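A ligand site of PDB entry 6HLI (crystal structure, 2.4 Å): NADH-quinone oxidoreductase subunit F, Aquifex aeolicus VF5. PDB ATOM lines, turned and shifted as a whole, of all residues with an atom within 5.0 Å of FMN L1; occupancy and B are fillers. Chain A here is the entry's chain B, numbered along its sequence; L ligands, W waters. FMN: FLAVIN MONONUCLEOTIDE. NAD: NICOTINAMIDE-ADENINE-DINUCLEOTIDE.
O of Val 218 lies within hydrogen-bond range of NZ of Lys 76, 2.7 Å away.
The side-chain hydroxyl (OG1) of Thr 223 is in hydrogen-bond range of the backbone NH (N) of Arg 66 (2.8 Å).
O of Arg 66 sits close to OD1 of Asn 220, at 3.5 Å.
The backbone NH of Asp 94 is in hydrogen-bond range of the side-chain amide oxygen of Asn 92 (3.3 Å).
N of Asp 103 is in hydrogen-bond range of OE2 of Glu 95 (2.8 Å).
O of Phe 71 is in hydrogen-bond range of N of Gly 65 (2.8 Å).
The backbone NH (N) of Gly 183 sits at hydrogen-bond distance from the side-chain carboxylate (OD2) of Asp 94.
O of Asp 94 sits at hydrogen-bond distance from OG of Ser 96.
O2N of NAD L2 sits at hydrogen-bond distance from O2' of FMN L1 (2.8 Å).
The backbone carbonyl oxygen (O) of Gly 183 lies close to a nitrogen (N10) of FMN L1 (3.3 Å).
Residues that only touch FMN L1: Gly 65 (3.1 Å), Asp 94 (3.4 Å), Glu 184 (3.5 Å), Val 218 (3.5 Å), Tyr 180 (3.5 Å), Ser 96 (3.7 Å), Ile 181 (3.8 Å) and Gly 394 (3.8 Å).
The nearest printed residue that does not touch FMN L1 is Leu 395 (4.1 Å).
The side-chain amino group (NZ) of Lys 76 lies within salt-bridge range of an oxygen (O2P) of FMN L1.
O3P of FMN L1 sits at hydrogen-bond distance from OG1 of Thr 223 (2.7 Å).
The backbone NH (N) of Asn 220 sits at hydrogen-bond distance from an oxygen (O3P) of FMN L1 (3.0 Å).
An oxygen (O2) of FMN L1 sits at hydrogen-bond distance from the side-chain amide nitrogen (ND2) of Asn 220.
The side-chain amide nitrogen (ND2) of Asn 219 sits at hydrogen-bond distance from an oxygen (O3P) of FMN L1, 2.8 Å away.
ND2 of Asn 92 is in hydrogen-bond range of O4' of FMN L1 (2.8 Å).
N of Gly 67 is in hydrogen-bond range of O1P of FMN L1 (2.8 Å).
An oxygen (O4) of FMN L1 sits at hydrogen-bond distance from the backbone NH of Glu 95, at 2.9 Å.
The backbone NH (N) of Glu 185 lies within hydrogen-bond range of an oxygen (O2') of FMN L1, 3.1 Å away.
N of Arg 66 lies within hydrogen-bond range of O1P of FMN L1, at 3.2 Å.
The side-chain amino group (NZ) of Lys 76 is in hydrogen-bond range of an oxygen (O3B) of NAD L2, at 2.7 Å.
The side-chain carboxylate of Glu 185 lies within hydrogen-bond range of an oxygen (O3B) of NAD L2 (2.7 Å).
An oxygen (O3D) of NAD L2 lies within hydrogen-bond range of the backbone carbonyl oxygen (O) of Gly 68, at 2.9 Å.
Water W4 lies within hydrogen-bond range of the backbone carbonyl oxygen of Phe 71 (2.7 Å), an oxygen (O2P) of FMN L1 (2.7 Å), the backbone NH of Gly 65 (3.1 Å) and the side-chain amide nitrogen of Asn 219 (3.3 Å).
Water W6 lies within hydrogen-bond range of N of Ala 69 (2.7 Å), O1P of FMN L1 (2.9 Å), O of Gly 67 (3.0 Å) and N of Gly 68 (3.4 Å).
Water W5 lies within hydrogen-bond range of N of Phe 71 (2.9 Å) and O2P of FMN L1 (2.9 Å).
Water W2 lies within hydrogen-bond range of an oxygen (O1N) of NAD L2 (2.7 Å), the backbone NH of Gly 394 (3.1 Å) and the side-chain carboxylate of Glu 184 (3.1 Å).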
ATOM      1  N   GLY A  65      -0.747  19.706 -14.797  1.00  0.00           N
ATOM      2  CA  GLY A  65      -1.084  19.560 -16.210  1.00  0.00           C
ATOM      3  C   GLY A  65      -2.570  19.508 -16.480  1.00  0.00           C
ATOM      4  O   GLY A  65      -3.311  18.828 -15.765  1.00  0.00           O
ATOM      5  N   ARG A  66      -3.013  20.284 -17.468  1.00  0.00           N
ATOM      6  CA  ARG A  66      -4.435  20.403 -17.830  1.00  0.00           C
ATOM      7  C   ARG A  66      -4.850  19.441 -18.962  1.00  0.00           C
ATOM      8  O   ARG A  66      -5.989  19.458 -19.428  1.00  0.00           O
ATOM      9  CB  ARG A  66      -4.791  21.865 -18.182  1.00  0.00           C
ATOM     10  CG  ARG A  66      -4.626  22.868 -17.032  1.00  0.00           C
ATOM     11  CD  ARG A  66      -5.521  22.589 -15.841  1.00  0.00           C
ATOM     12  NE  ARG A  66      -5.559  23.741 -14.937  1.00  0.00           N
ATOM     13  CZ  ARG A  66      -5.055  23.762 -13.710  1.00  0.00           C
ATOM     14  NH1 ARG A  66      -5.140  24.865 -12.971  1.00  0.00           N
ATOM     15  NH2 ARG A  66      -4.481  22.671 -13.190  1.00  0.00           N
ATOM     16  N   GLY A  67      -3.915  18.615 -19.393  1.00  0.00           N
ATOM     17  CA  GLY A  67      -4.163  17.659 -20.474  1.00  0.00           C
ATOM     18  C   GLY A  67      -4.617  16.304 -19.981  1.00  0.00           C
ATOM     19  O   GLY A  67      -4.360  15.308 -20.662  1.00  0.00           O
ATOM     20  N   GLY A  68      -5.222  16.234 -18.791  1.00  0.00           N
ATOM     21  CA  GLY A  68      -5.805  15.013 -18.239  1.00  0.00           C
ATOM     22  C   GLY A  68      -5.115  14.224 -17.151  1.00  0.00           C
ATOM     23  O   GLY A  68      -5.797  13.623 -16.318  1.00  0.00           O
ATOM     24  N   ALA A  69      -3.786  14.124 -17.183  1.00  0.00           N
ATOM     25  CA  ALA A  69      -3.047  13.343 -16.203  1.00  0.00           C
ATOM     26  C   ALA A  69      -2.686  14.112 -14.913  1.00  0.00           C
ATOM     27  O   ALA A  69      -2.338  13.492 -13.907  1.00  0.00           O
ATOM     28  CB  ALA A  69      -1.824  12.735 -16.849  1.00  0.00           C
ATOM     29  N   PHE A  71      -0.070  16.104 -13.968  1.00  0.00           N
ATOM     30  CA  PHE A  71       1.298  16.046 -13.426  1.00  0.00           C
ATOM     31  C   PHE A  71       1.788  17.465 -13.024  1.00  0.00           C
ATOM     32  O   PHE A  71       1.513  18.407 -13.770  1.00  0.00           O
ATOM     33  CB  PHE A  71       2.252  15.427 -14.448  1.00  0.00           C
ATOM     34  CG  PHE A  71       3.604  15.038 -13.909  1.00  0.00           C
ATOM     35  CD1 PHE A  71       3.783  13.831 -13.256  1.00  0.00           C
ATOM     36  CD2 PHE A  71       4.688  15.881 -14.067  1.00  0.00           C
ATOM     37  CE1 PHE A  71       5.034  13.484 -12.748  1.00  0.00           C
ATOM     38  CE2 PHE A  71       5.951  15.525 -13.552  1.00  0.00           C
ATOM     39  CZ  PHE A  71       6.109  14.324 -12.896  1.00  0.00           C
ATOM     40  N   LYS A  76       7.838  18.749 -13.738  1.00  0.00           N
ATOM     41  CA  LYS A  76       8.162  18.336 -15.106  1.00  0.00           C
ATOM     42  C   LYS A  76       9.318  19.160 -15.706  1.00  0.00           C
ATOM     43  O   LYS A  76      10.212  18.588 -16.314  1.00  0.00           O
ATOM     44  CB  LYS A  76       6.931  18.400 -16.012  1.00  0.00           C
ATOM     45  CG  LYS A  76       7.086  17.541 -17.280  1.00  0.00           C
ATOM     46  CD  LYS A  76       6.039  17.854 -18.372  1.00  0.00           C
ATOM     47  CE  LYS A  76       4.644  17.436 -17.939  1.00  0.00           C
ATOM     48  NZ  LYS A  76       3.730  17.358 -19.083  1.00  0.00           N
ATOM     49  N   ASN A  92       0.867  21.039 -26.592  1.00  0.00           N
ATOM     50  CA  ASN A  92      -0.071  20.012 -27.035  1.00  0.00           C
ATOM     51  C   ASN A  92      -1.447  20.640 -27.388  1.00  0.00           C
ATOM     52  O   ASN A  92      -2.273  20.913 -26.501  1.00  0.00           O
ATOM     53  CB  ASN A  92      -0.208  18.893 -26.010  1.00  0.00           C
ATOM     54  CG  ASN A  92      -0.664  17.579 -26.614  1.00  0.00           C
ATOM     55  OD1 ASN A  92      -1.428  17.546 -27.606  1.00  0.00           O
ATOM     56  ND2 ASN A  92      -0.142  16.454 -26.062  1.00  0.00           N
ATOM     57  N   ASP A  94      -3.575  19.095 -29.545  1.00  0.00           N
ATOM     58  CA  ASP A  94      -4.216  18.014 -30.280  1.00  0.00           C
ATOM     59  C   ASP A  94      -5.707  17.805 -29.942  1.00  0.00           C
ATOM     60  O   ASP A  94      -6.441  17.373 -30.811  1.00  0.00           O
ATOM     61  CB  ASP A  94      -3.420  16.712 -30.151  1.00  0.00           C
ATOM     62  CG  ASP A  94      -3.740  15.741 -31.266  1.00  0.00           C
ATOM     63  OD1 ASP A  94      -3.351  16.018 -32.423  1.00  0.00           O
ATOM     64  OD2 ASP A  94      -4.441  14.750 -30.997  1.00  0.00           O
ATOM     65  N   GLU A  95      -6.158  18.157 -28.732  1.00  0.00           N
ATOM     66  CA  GLU A  95      -7.553  18.076 -28.232  1.00  0.00           C
ATOM     67  C   GLU A  95      -8.566  17.289 -29.135  1.00  0.00           C
ATOM     68  O   GLU A  95      -9.287  17.885 -29.935  1.00  0.00           O
ATOM     69  CB  GLU A  95      -8.081  19.500 -27.914  1.00  0.00           C
ATOM     70  CG  GLU A  95      -9.371  19.505 -27.126  1.00  0.00           C
ATOM     71  CD  GLU A  95      -9.833  20.883 -26.733  1.00  0.00           C
ATOM     72  OE1 GLU A  95     -10.170  21.681 -27.639  1.00  0.00           O
ATOM     73  OE2 GLU A  95      -9.876  21.173 -25.524  1.00  0.00           O
ATOM     74  N   SER A  96      -8.563  15.970 -29.011  1.00  0.00           N
ATOM     75  CA  SER A  96      -9.400  15.053 -29.795  1.00  0.00           C
ATOM     76  C   SER A  96     -10.337  14.194 -28.891  1.00  0.00           C
ATOM     77  O   SER A  96     -11.114  13.379 -29.401  1.00  0.00           O
ATOM     78  CB  SER A  96      -8.534  14.174 -30.708  1.00  0.00           C
ATOM     79  OG  SER A  96      -7.638  14.874 -31.572  1.00  0.00           O
ATOM     80  N   ASP A 103      -9.507  23.907 -24.987  1.00  0.00           N
ATOM     81  CA  ASP A 103      -8.253  24.428 -25.538  1.00  0.00           C
ATOM     82  C   ASP A 103      -8.495  25.312 -26.769  1.00  0.00           C
ATOM     83  O   ASP A 103      -7.860  26.358 -26.887  1.00  0.00           O
ATOM     84  CB  ASP A 103      -7.291  23.298 -25.912  1.00  0.00           C
ATOM     85  CG  ASP A 103      -6.807  22.443 -24.748  1.00  0.00           C
ATOM     86  OD1 ASP A 103      -6.972  22.871 -23.602  1.00  0.00           O
ATOM     87  OD2 ASP A 103      -6.259  21.368 -24.989  1.00  0.00           O
ATOM     88  N   TYR A 180      -6.200  10.598 -33.109  1.00  0.00           N
ATOM     89  CA  TYR A 180      -6.393  10.876 -31.679  1.00  0.00           C
ATOM     90  C   TYR A 180      -5.145  10.550 -30.849  1.00  0.00           C
ATOM     91  O   TYR A 180      -4.788  11.308 -29.939  1.00  0.00           O
ATOM     92  CB  TYR A 180      -7.590  10.078 -31.140  1.00  0.00           C
ATOM     93  CG  TYR A 180      -7.687  10.016 -29.636  1.00  0.00           C
ATOM     94  CD1 TYR A 180      -7.973  11.161 -28.896  1.00  0.00           C
ATOM     95  CD2 TYR A 180      -7.487   8.826 -28.942  1.00  0.00           C
ATOM     96  CE1 TYR A 180      -8.066  11.131 -27.499  1.00  0.00           C
ATOM     97  CE2 TYR A 180      -7.606   8.763 -27.558  1.00  0.00           C
ATOM     98  CZ  TYR A 180      -7.876   9.924 -26.837  1.00  0.00           C
ATOM     99  OH  TYR A 180      -7.985   9.917 -25.466  1.00  0.00           O
ATOM    100  N   ILE A 181      -4.494   9.423 -31.163  1.00  0.00           N
ATOM    101  CA  ILE A 181      -3.287   8.939 -30.509  1.00  0.00           C
ATOM    102  C   ILE A 181      -2.131   9.957 -30.555  1.00  0.00           C
ATOM    103  O   ILE A 181      -1.251   9.899 -29.695  1.00  0.00           O
ATOM    104  CB  ILE A 181      -2.902   7.544 -31.099  1.00  0.00           C
ATOM    105  CG1 ILE A 181      -1.966   6.719 -30.162  1.00  0.00           C
ATOM    106  CG2 ILE A 181      -2.315   7.645 -32.526  1.00  0.00           C
ATOM    107  CD1 ILE A 181      -2.402   6.622 -28.743  1.00  0.00           C
ATOM    108  N   GLY A 183      -2.139  12.866 -29.726  1.00  0.00           N
ATOM    109  CA  GLY A 183      -2.269  13.705 -28.546  1.00  0.00           C
ATOM    110  C   GLY A 183      -1.430  13.129 -27.431  1.00  0.00           C
ATOM    111  O   GLY A 183      -1.043  13.847 -26.500  1.00  0.00           O
ATOM    112  N   GLU A 184      -1.167  11.801 -27.484  1.00  0.00           N
ATOM    113  CA  GLU A 184      -0.279  11.134 -26.554  1.00  0.00           C
ATOM    114  C   GLU A 184       1.128  11.704 -26.912  1.00  0.00           C
ATOM    115  O   GLU A 184       1.537  11.678 -28.083  1.00  0.00           O
ATOM    116  CB  GLU A 184      -0.367   9.604 -26.699  1.00  0.00           C
ATOM    117  CG  GLU A 184       0.341   8.828 -25.611  1.00  0.00           C
ATOM    118  CD  GLU A 184       1.837   8.686 -25.774  1.00  0.00           C
ATOM    119  OE1 GLU A 184       2.329   8.730 -26.923  1.00  0.00           O
ATOM    120  OE2 GLU A 184       2.526   8.534 -24.732  1.00  0.00           O
ATOM    121  N   GLU A 185       1.794  12.301 -25.935  1.00  0.00           N
ATOM    122  CA  GLU A 185       3.064  13.016 -26.078  1.00  0.00           C
ATOM    123  C   GLU A 185       4.161  12.368 -26.940  1.00  0.00           C
ATOM    124  O   GLU A 185       4.736  13.071 -27.752  1.00  0.00           O
ATOM    125  CB  GLU A 185       3.637  13.371 -24.711  1.00  0.00           C
ATOM    126  CG  GLU A 185       3.787  12.190 -23.785  1.00  0.00           C
ATOM    127  CD  GLU A 185       4.474  12.546 -22.493  1.00  0.00           C
ATOM    128  OE1 GLU A 185       4.611  13.758 -22.204  1.00  0.00           O
ATOM    129  OE2 GLU A 185       4.889  11.602 -21.785  1.00  0.00           O
ATOM    130  N   VAL A 218       6.534  18.610 -22.917  1.00  0.00           N
ATOM    131  CA  VAL A 218       5.242  18.647 -23.564  1.00  0.00           C
ATOM    132  C   VAL A 218       4.212  19.112 -22.548  1.00  0.00           C
ATOM    133  O   VAL A 218       4.103  18.506 -21.492  1.00  0.00           O
ATOM    134  CB  VAL A 218       4.817  17.335 -24.263  1.00  0.00           C
ATOM    135  CG1 VAL A 218       3.538  17.558 -25.065  1.00  0.00           C
ATOM    136  CG2 VAL A 218       5.950  16.805 -25.171  1.00  0.00           C
ATOM    137  N   ASN A 219       3.500  20.235 -22.861  1.00  0.00           N
ATOM    138  CA  ASN A 219       2.440  20.786 -22.000  1.00  0.00           C
ATOM    139  C   ASN A 219       1.223  21.107 -22.834  1.00  0.00           C
ATOM    140  O   ASN A 219       1.364  21.393 -24.020  1.00  0.00           O
ATOM    141  CB  ASN A 219       2.900  22.004 -21.209  1.00  0.00           C
ATOM    142  CG  ASN A 219       3.585  21.683 -19.878  1.00  0.00           C
ATOM    143  OD1 ASN A 219       4.729  22.109 -19.624  1.00  0.00           O
ATOM    144  ND2 ASN A 219       2.912  20.940 -18.988  1.00  0.00           N
ATOM    145  N   ASN A 220       0.050  20.980 -22.236  1.00  0.00           N
ATOM    146  CA  ASN A 220      -1.274  21.236 -22.812  1.00  0.00           C
ATOM    147  C   ASN A 220      -1.511  22.742 -22.916  1.00  0.00           C
ATOM    148  O   ASN A 220      -1.023  23.478 -22.057  1.00  0.00           O
ATOM    149  CB  ASN A 220      -2.346  20.589 -21.886  1.00  0.00           C
ATOM    150  CG  ASN A 220      -3.765  20.941 -22.229  1.00  0.00           C
ATOM    151  OD1 ASN A 220      -4.415  21.726 -21.565  1.00  0.00           O
ATOM    152  ND2 ASN A 220      -4.251  20.414 -23.320  1.00  0.00           N
ATOM    153  N   THR A 223      -2.642  24.494 -19.748  1.00  0.00           N
ATOM    154  CA  THR A 223      -1.555  24.553 -18.742  1.00  0.00           C
ATOM    155  C   THR A 223      -0.677  25.789 -18.962  1.00  0.00           C
ATOM    156  O   THR A 223      -0.451  26.560 -18.012  1.00  0.00           O
ATOM    157  CB  THR A 223      -0.669  23.278 -18.793  1.00  0.00           C
ATOM    158  OG1 THR A 223      -1.486  22.108 -18.979  1.00  0.00           O
ATOM    159  CG2 THR A 223       0.249  23.138 -17.574  1.00  0.00           C
ATOM    160  N   CYS A 393       0.889   2.588 -24.046  1.00  0.00           N
ATOM    161  CA  CYS A 393       0.345   3.926 -23.833  1.00  0.00           C
ATOM    162  C   CYS A 393      -1.027   3.884 -23.135  1.00  0.00           C
ATOM    163  O   CYS A 393      -1.650   2.814 -23.042  1.00  0.00           O
ATOM    164  CB  CYS A 393       0.331   4.761 -25.111  1.00  0.00           C
ATOM    165  SG  CYS A 393      -1.267   4.861 -25.954  1.00  0.00           S
ATOM    166  N   GLY A 394      -1.421   5.023 -22.565  1.00  0.00           N
ATOM    167  CA  GLY A 394      -2.654   5.217 -21.804  1.00  0.00           C
ATOM    168  C   GLY A 394      -3.948   4.828 -22.482  1.00  0.00           C
ATOM    169  O   GLY A 394      -4.943   4.607 -21.790  1.00  0.00           O
ATOM    170  N   LEU A 395      -3.962   4.722 -23.848  1.00  0.00           N
ATOM    171  CA  LEU A 395      -5.145   4.347 -24.619  1.00  0.00           C
ATOM    172  C   LEU A 395      -5.646   2.941 -24.282  1.00  0.00           C
ATOM    173  O   LEU A 395      -6.835   2.788 -23.993  1.00  0.00           O
ATOM    174  CB  LEU A 395      -4.921   4.484 -26.148  1.00  0.00           C
ATOM    175  CG  LEU A 395      -6.190   4.548 -27.028  1.00  0.00           C
ATOM    176  CD1 LEU A 395      -5.948   5.404 -28.264  1.00  0.00           C
ATOM    177  CD2 LEU A 395      -6.710   3.140 -27.404  1.00  0.00           C
HETATM  178  N1  FMN L   1      -2.890  15.907 -23.854  1.00  0.00           N
HETATM  179  C2  FMN L   1      -3.300  17.052 -24.477  1.00  0.00           C
HETATM  180  O2  FMN L   1      -2.865  18.156 -24.142  1.00  0.00           O
HETATM  181  N3  FMN L   1      -4.130  16.980 -25.590  1.00  0.00           N
HETATM  182  C4  FMN L   1      -4.574  15.825 -26.209  1.00  0.00           C
HETATM  183  O4  FMN L   1      -5.360  15.891 -27.141  1.00  0.00           O
HETATM  184  C4A FMN L   1      -4.080  14.601 -25.589  1.00  0.00           C
HETATM  185  N5  FMN L   1      -4.388  13.464 -26.141  1.00  0.00           N
HETATM  186  C5A FMN L   1      -3.962  12.289 -25.514  1.00  0.00           C
HETATM  187  C6  FMN L   1      -4.328  11.065 -26.083  1.00  0.00           C
HETATM  188  C7  FMN L   1      -3.981   9.861 -25.472  1.00  0.00           C
HETATM  189  C7M FMN L   1      -4.363   8.558 -26.134  1.00  0.00           C
HETATM  190  C8  FMN L   1      -3.244   9.880 -24.264  1.00  0.00           C
HETATM  191  C8M FMN L   1      -2.815   8.601 -23.573  1.00  0.00           C
HETATM  192  C9  FMN L   1      -2.858  11.100 -23.708  1.00  0.00           C
HETATM  193  C9A FMN L   1      -3.206  12.304 -24.320  1.00  0.00           C
HETATM  194  N10 FMN L   1      -2.828  13.566 -23.776  1.00  0.00           N
HETATM  195  C10 FMN L   1      -3.251  14.737 -24.384  1.00  0.00           C
HETATM  196  C1' FMN L   1      -1.890  13.619 -22.640  1.00  0.00           C
HETATM  197  C2' FMN L   1      -0.435  13.792 -23.091  1.00  0.00           C
HETATM  198  O2' FMN L   1       0.170  12.508 -23.323  1.00  0.00           O
HETATM  199  C3' FMN L   1       0.402  14.596 -22.091  1.00  0.00           C
HETATM  200  O3' FMN L   1       0.327  13.991 -20.793  1.00  0.00           O
HETATM  201  C4' FMN L   1       0.075  16.090 -21.981  1.00  0.00           C
HETATM  202  O4' FMN L   1       0.016  16.714 -23.269  1.00  0.00           O
HETATM  203  C5' FMN L   1       1.099  16.794 -21.123  1.00  0.00           C
HETATM  204  O5' FMN L   1       0.676  18.133 -20.813  1.00  0.00           O
HETATM  205  P   FMN L   1       0.221  18.599 -19.338  1.00  0.00           P
HETATM  206  O1P FMN L   1      -1.184  18.103 -18.937  1.00  0.00           O
HETATM  207  O2P FMN L   1       1.275  18.138 -18.333  1.00  0.00           O
HETATM  208  O3P FMN L   1       0.270  20.121 -19.404  1.00  0.00           O
HETATM  209  PA  NAD L   2       0.869  10.233 -17.551  1.00  0.00           P
HETATM  210  O1A NAD L   2       0.294  10.085 -16.195  1.00  0.00           O
HETATM  211  O2A NAD L   2       1.672   8.980 -17.895  1.00  0.00           O
HETATM  212  O5B NAD L   2       1.940  11.439 -17.627  1.00  0.00           O
HETATM  213  C5B NAD L   2       1.535  12.812 -17.701  1.00  0.00           C
HETATM  214  C4B NAD L   2       2.723  13.708 -17.946  1.00  0.00           C
HETATM  215  O4B NAD L   2       3.666  13.578 -16.871  1.00  0.00           O
HETATM  216  C3B NAD L   2       3.508  13.496 -19.247  1.00  0.00           C
HETATM  217  O3B NAD L   2       3.784  14.746 -19.868  1.00  0.00           O
HETATM  218  C2B NAD L   2       4.810  12.819 -18.800  1.00  0.00           C
HETATM  219  O2B NAD L   2       5.961  13.159 -19.563  1.00  0.00           O
HETATM  220  C1B NAD L   2       4.967  13.314 -17.367  1.00  0.00           C
HETATM  221  N9A NAD L   2       5.586  12.339 -16.496  1.00  0.00           N
HETATM  222  C8A NAD L   2       4.971  11.324 -15.813  1.00  0.00           C
HETATM  223  N7A NAD L   2       5.776  10.641 -15.028  1.00  0.00           N
HETATM  224  C5A NAD L   2       7.008  11.255 -15.214  1.00  0.00           C
HETATM  225  C6A NAD L   2       8.276  11.007 -14.670  1.00  0.00           C
HETATM  226  N6A NAD L   2       8.515  10.085 -13.732  1.00  0.00           N
HETATM  227  N1A NAD L   2       9.316  11.772 -15.102  1.00  0.00           N
HETATM  228  C2A NAD L   2       9.073  12.729 -16.014  1.00  0.00           C
HETATM  229  N3A NAD L   2       7.909  13.071 -16.585  1.00  0.00           N
HETATM  230  C4A NAD L   2       6.915  12.288 -16.131  1.00  0.00           C
HETATM  231  O3  NAD L   2      -0.354  10.431 -18.559  1.00  0.00           O
HETATM  232  PN  NAD L   2      -0.641  10.260 -20.125  1.00  0.00           P
HETATM  233  O1N NAD L   2      -0.644   8.809 -20.400  1.00  0.00           O
HETATM  234  O2N NAD L   2       0.298  11.139 -20.862  1.00  0.00           O
HETATM  235  O5D NAD L   2      -2.091  10.931 -20.329  1.00  0.00           O
HETATM  236  C5D NAD L   2      -3.392  10.360 -20.045  1.00  0.00           C
HETATM  237  C4D NAD L   2      -4.413  11.464 -19.903  1.00  0.00           C
HETATM  238  O4D NAD L   2      -4.575  12.168 -21.154  1.00  0.00           O
HETATM  239  C3D NAD L   2      -5.841  11.062 -19.473  1.00  0.00           C
HETATM  240  O3D NAD L   2      -6.149  11.323 -18.102  1.00  0.00           O
HETATM  241  C2D NAD L   2      -6.765  11.886 -20.392  1.00  0.00           C
HETATM  242  O2D NAD L   2      -7.753  12.634 -19.701  1.00  0.00           O
HETATM  243  C1D NAD L   2      -5.803  12.833 -21.090  1.00  0.00           C
HETATM  244  N1N NAD L   2      -6.238  13.235 -22.541  1.00  0.00           N
HETATM  245  C2N NAD L   2      -6.483  14.543 -22.750  1.00  0.00           C
HETATM  246  C3N NAD L   2      -7.057  14.957 -23.936  1.00  0.00           C
HETATM  247  C7N NAD L   2      -7.385  16.411 -24.221  1.00  0.00           C
HETATM  248  O7N NAD L   2      -7.891  16.716 -25.322  1.00  0.00           O
HETATM  249  N7N NAD L   2      -7.121  17.306 -23.296  1.00  0.00           N
HETATM  250  C4N NAD L   2      -7.374  13.998 -24.895  1.00  0.00           C
HETATM  251  C5N NAD L   2      -7.112  12.665 -24.653  1.00  0.00           C
HETATM  252  C6N NAD L   2      -6.525  12.296 -23.471  1.00  0.00           C
HETATM  253  O   HOH W   1      -5.804  13.588 -28.935  1.00  0.00           O
HETATM  254  O   HOH W   2       0.348   7.624 -22.647  1.00  0.00           O
HETATM  255  O   HOH W   3      -4.717  19.770 -26.292  1.00  0.00           O
HETATM  256  O   HOH W   4       2.056  19.541 -16.131  1.00  0.00           O
HETATM  257  O   HOH W   5       0.077  15.925 -16.838  1.00  0.00           O
HETATM  258  O   HOH W   6      -1.943  15.340 -18.816  1.00  0.00           O
